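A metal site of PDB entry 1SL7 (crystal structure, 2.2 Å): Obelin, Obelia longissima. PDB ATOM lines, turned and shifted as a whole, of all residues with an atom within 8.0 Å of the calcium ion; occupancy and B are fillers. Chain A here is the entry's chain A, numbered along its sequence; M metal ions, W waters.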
ATOM      1  N   PHE A 119     -15.905 -17.673 -24.324  1.00  0.00           N
ATOM      2  CA  PHE A 119     -16.943 -17.793 -25.361  1.00  0.00           C
ATOM      3  C   PHE A 119     -18.370 -17.995 -24.773  1.00  0.00           C
ATOM      4  O   PHE A 119     -19.325 -17.317 -25.179  1.00  0.00           O
ATOM      5  CB  PHE A 119     -16.589 -18.936 -26.314  1.00  0.00           C
ATOM      6  CG  PHE A 119     -17.268 -18.861 -27.666  1.00  0.00           C
ATOM      7  CD1 PHE A 119     -16.735 -18.071 -28.671  1.00  0.00           C
ATOM      8  CD2 PHE A 119     -18.440 -19.594 -27.918  1.00  0.00           C
ATOM      9  CE1 PHE A 119     -17.370 -18.002 -29.931  1.00  0.00           C
ATOM     10  CE2 PHE A 119     -19.076 -19.528 -29.164  1.00  0.00           C
ATOM     11  CZ  PHE A 119     -18.538 -18.726 -30.173  1.00  0.00           C
ATOM     12  N   PHE A 122     -19.868 -14.560 -23.298  1.00  0.00           N
ATOM     13  CA  PHE A 122     -20.255 -13.595 -24.322  1.00  0.00           C
ATOM     14  C   PHE A 122     -21.511 -14.012 -25.141  1.00  0.00           C
ATOM     15  O   PHE A 122     -22.204 -13.139 -25.664  1.00  0.00           O
ATOM     16  CB  PHE A 122     -19.094 -13.367 -25.311  1.00  0.00           C
ATOM     17  CG  PHE A 122     -18.046 -12.365 -24.834  1.00  0.00           C
ATOM     18  CD1 PHE A 122     -18.134 -11.021 -25.187  1.00  0.00           C
ATOM     19  CD2 PHE A 122     -16.952 -12.798 -24.064  1.00  0.00           C
ATOM     20  CE1 PHE A 122     -17.167 -10.099 -24.766  1.00  0.00           C
ATOM     21  CE2 PHE A 122     -15.969 -11.883 -23.642  1.00  0.00           C
ATOM     22  CZ  PHE A 122     -16.080 -10.534 -23.990  1.00  0.00           C
ATOM     23  N   ASP A 123     -21.761 -15.311 -25.259  1.00  0.00           N
ATOM     24  CA  ASP A 123     -22.856 -15.859 -26.089  1.00  0.00           C
ATOM     25  C   ASP A 123     -24.161 -15.920 -25.276  1.00  0.00           C
ATOM     26  O   ASP A 123     -24.579 -16.991 -24.863  1.00  0.00           O
ATOM     27  CB  ASP A 123     -22.467 -17.260 -26.637  1.00  0.00           C
ATOM     28  CG  ASP A 123     -23.482 -17.831 -27.665  1.00  0.00           C
ATOM     29  OD1 ASP A 123     -24.276 -17.071 -28.252  1.00  0.00           O
ATOM     30  OD2 ASP A 123     -23.535 -19.065 -27.941  1.00  0.00           O
ATOM     31  N   LYS A 124     -24.770 -14.754 -25.056  1.00  0.00           N
ATOM     32  CA  LYS A 124     -25.948 -14.594 -24.183  1.00  0.00           C
ATOM     33  C   LYS A 124     -27.192 -15.385 -24.607  1.00  0.00           C
ATOM     34  O   LYS A 124     -27.825 -16.023 -23.761  1.00  0.00           O
ATOM     35  CB  LYS A 124     -26.298 -13.110 -23.962  1.00  0.00           C
ATOM     36  CG  LYS A 124     -25.356 -12.349 -23.037  1.00  0.00           C
ATOM     37  CD  LYS A 124     -25.187 -13.031 -21.681  1.00  0.00           C
ATOM     38  CE  LYS A 124     -24.402 -12.153 -20.711  1.00  0.00           C
ATOM     39  NZ  LYS A 124     -24.590 -12.613 -19.307  1.00  0.00           N
ATOM     40  N   ASP A 125     -27.564 -15.344 -25.890  1.00  0.00           N
ATOM     41  CA  ASP A 125     -28.601 -16.270 -26.372  1.00  0.00           C
ATOM     42  C   ASP A 125     -27.942 -17.633 -26.471  1.00  0.00           C
ATOM     43  O   ASP A 125     -26.921 -17.852 -25.829  1.00  0.00           O
ATOM     44  CB  ASP A 125     -29.267 -15.814 -27.699  1.00  0.00           C
ATOM     45  CG  ASP A 125     -28.272 -15.515 -28.811  1.00  0.00           C
ATOM     46  OD1 ASP A 125     -27.142 -16.057 -28.820  1.00  0.00           O
ATOM     47  OD2 ASP A 125     -28.545 -14.719 -29.738  1.00  0.00           O
ATOM     48  N   GLY A 126     -28.497 -18.573 -27.227  1.00  0.00           N
ATOM     49  CA  GLY A 126     -27.828 -19.869 -27.283  1.00  0.00           C
ATOM     50  C   GLY A 126     -27.186 -20.202 -28.608  1.00  0.00           C
ATOM     51  O   GLY A 126     -27.018 -21.376 -28.923  1.00  0.00           O
ATOM     52  N   SER A 127     -26.813 -19.173 -29.376  1.00  0.00           N
ATOM     53  CA  SER A 127     -26.593 -19.299 -30.817  1.00  0.00           C
ATOM     54  C   SER A 127     -25.287 -19.992 -31.261  1.00  0.00           C
ATOM     55  O   SER A 127     -25.236 -20.583 -32.350  1.00  0.00           O
ATOM     56  CB  SER A 127     -26.766 -17.946 -31.506  1.00  0.00           C
ATOM     57  OG  SER A 127     -25.646 -17.096 -31.275  1.00  0.00           O
ATOM     58  N   GLY A 128     -24.238 -19.923 -30.458  1.00  0.00           N
ATOM     59  CA  GLY A 128     -22.981 -20.566 -30.826  1.00  0.00           C
ATOM     60  C   GLY A 128     -22.072 -19.696 -31.686  1.00  0.00           C
ATOM     61  O   GLY A 128     -21.061 -20.180 -32.178  1.00  0.00           O
ATOM     62  N   THR A 129     -22.452 -18.429 -31.859  1.00  0.00           N
ATOM     63  CA  THR A 129     -21.632 -17.422 -32.537  1.00  0.00           C
ATOM     64  C   THR A 129     -21.756 -16.102 -31.752  1.00  0.00           C
ATOM     65  O   THR A 129     -22.761 -15.876 -31.069  1.00  0.00           O
ATOM     66  CB  THR A 129     -22.144 -17.176 -33.972  1.00  0.00           C
ATOM     67  OG1 THR A 129     -23.512 -16.740 -33.913  1.00  0.00           O
ATOM     68  CG2 THR A 129     -22.219 -18.474 -34.808  1.00  0.00           C
ATOM     69  N   ILE A 130     -20.750 -15.224 -31.871  1.00  0.00           N
ATOM     70  CA  ILE A 130     -20.790 -13.889 -31.261  1.00  0.00           C
ATOM     71  C   ILE A 130     -21.092 -12.813 -32.297  1.00  0.00           C
ATOM     72  O   ILE A 130     -20.375 -12.689 -33.305  1.00  0.00           O
ATOM     73  CB  ILE A 130     -19.449 -13.557 -30.521  1.00  0.00           C
ATOM     74  CG1 ILE A 130     -18.968 -14.729 -29.633  1.00  0.00           C
ATOM     75  CG2 ILE A 130     -19.582 -12.242 -29.716  1.00  0.00           C
ATOM     76  CD1 ILE A 130     -19.919 -15.140 -28.544  1.00  0.00           C
ATOM     77  N   THR A 131     -22.146 -12.031 -32.027  1.00  0.00           N
ATOM     78  CA  THR A 131     -22.533 -10.890 -32.873  1.00  0.00           C
ATOM     79  C   THR A 131     -22.116  -9.560 -32.255  1.00  0.00           C
ATOM     80  O   THR A 131     -21.684  -9.497 -31.090  1.00  0.00           O
ATOM     81  CB  THR A 131     -24.065 -10.887 -33.188  1.00  0.00           C
ATOM     82  OG1 THR A 131     -24.821 -11.134 -31.991  1.00  0.00           O
ATOM     83  CG2 THR A 131     -24.454 -12.046 -34.110  1.00  0.00           C
ATOM     84  N   LEU A 132     -22.277  -8.489 -33.033  1.00  0.00           N
ATOM     85  CA  LEU A 132     -21.781  -7.162 -32.674  1.00  0.00           C
ATOM     86  C   LEU A 132     -22.325  -6.623 -31.355  1.00  0.00           C
ATOM     87  O   LEU A 132     -21.582  -6.012 -30.573  1.00  0.00           O
ATOM     88  CB  LEU A 132     -22.064  -6.175 -33.827  1.00  0.00           C
ATOM     89  CG  LEU A 132     -21.513  -4.742 -33.730  1.00  0.00           C
ATOM     90  CD1 LEU A 132     -19.988  -4.708 -33.634  1.00  0.00           C
ATOM     91  CD2 LEU A 132     -22.017  -3.887 -34.908  1.00  0.00           C
ATOM     92  N   ASP A 133     -23.616  -6.847 -31.095  1.00  0.00           N
ATOM     93  CA  ASP A 133     -24.262  -6.396 -29.864  1.00  0.00           C
ATOM     94  C   ASP A 133     -23.684  -7.102 -28.626  1.00  0.00           C
ATOM     95  O   ASP A 133     -23.479  -6.473 -27.591  1.00  0.00           O
ATOM     96  CB  ASP A 133     -25.784  -6.597 -29.941  1.00  0.00           C
ATOM     97  CG  ASP A 133     -26.177  -8.033 -30.330  1.00  0.00           C
ATOM     98  OD1 ASP A 133     -25.587  -8.606 -31.272  1.00  0.00           O
ATOM     99  OD2 ASP A 133     -27.081  -8.670 -29.743  1.00  0.00           O
ATOM    100  N   GLU A 134     -23.416  -8.401 -28.757  1.00  0.00           N
ATOM    101  CA  GLU A 134     -22.812  -9.199 -27.678  1.00  0.00           C
ATOM    102  C   GLU A 134     -21.359  -8.788 -27.395  1.00  0.00           C
ATOM    103  O   GLU A 134     -20.948  -8.689 -26.225  1.00  0.00           O
ATOM    104  CB  GLU A 134     -22.901 -10.701 -27.997  1.00  0.00           C
ATOM    105  CG  GLU A 134     -24.338 -11.246 -28.021  1.00  0.00           C
ATOM    106  CD  GLU A 134     -24.442 -12.697 -28.476  1.00  0.00           C
ATOM    107  OE1 GLU A 134     -23.647 -13.141 -29.331  1.00  0.00           O
ATOM    108  OE2 GLU A 134     -25.337 -13.403 -27.960  1.00  0.00           O
ATOM    109  N   ASP A 165     -20.285 -12.718 -38.157  1.00  0.00           N
ATOM    110  CA  ASP A 165     -20.186 -13.054 -36.728  1.00  0.00           C
ATOM    111  C   ASP A 165     -18.845 -13.730 -36.373  1.00  0.00           C
ATOM    112  O   ASP A 165     -18.021 -13.965 -37.270  1.00  0.00           O
ATOM    113  CB  ASP A 165     -21.379 -13.939 -36.293  1.00  0.00           C
ATOM    114  CG  ASP A 165     -21.623 -15.118 -37.236  1.00  0.00           C
ATOM    115  OD1 ASP A 165     -20.730 -15.469 -38.038  1.00  0.00           O
ATOM    116  OD2 ASP A 165     -22.682 -15.779 -37.234  1.00  0.00           O
ATOM    117  N   LEU A 166     -18.614 -14.016 -35.091  1.00  0.00           N
ATOM    118  CA  LEU A 166     -17.346 -14.654 -34.680  1.00  0.00           C
ATOM    119  C   LEU A 166     -17.467 -16.104 -34.186  1.00  0.00           C
ATOM    120  O   LEU A 166     -18.313 -16.420 -33.348  1.00  0.00           O
ATOM    121  CB  LEU A 166     -16.585 -13.805 -33.631  1.00  0.00           C
ATOM    122  CG  LEU A 166     -16.467 -12.283 -33.821  1.00  0.00           C
ATOM    123  CD1 LEU A 166     -15.882 -11.645 -32.582  1.00  0.00           C
ATOM    124  CD2 LEU A 166     -15.654 -11.893 -35.070  1.00  0.00           C
HETATM  125 CA    CA M   1     -24.900 -15.282 -29.779  1.00  0.00          CA
HETATM  126  O   HOH W   1     -26.286 -13.924 -31.409  1.00  0.00           O
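Water W1 lies within hydrogen-bond range of the side-chain carboxylate of Asp 125 and the side-chain hydroxyl of Thr 131.
The calcium ion is bound by the side-chain carboxylate (OD1) of Asp 123 (2.4 Å), the side-chain hydroxyl (OG) of Ser 127 (2.5 Å), the side-chain carboxylate (OE1) of Glu 134 (2.5 Å), water W1 (2.5 Å), the side-chain carboxylate (OD1) of Asp 125 (2.6 Å), the backbone carbonyl oxygen (O) of Thr 129 (2.6 Å) and the side-chain carboxylate (OE2) of Glu 134 (2.7 Å).
OE2 of Glu 134 lies close to N of Lys 124.
OE1 of Glu 134 lies close to N of Thr 131, at 3.3 Å.
The side-chain carboxylate (OD2) of Asp 123 lies within hydrogen-bond range of the backbone NH (N) of Gly 128, 2.8 Å away.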
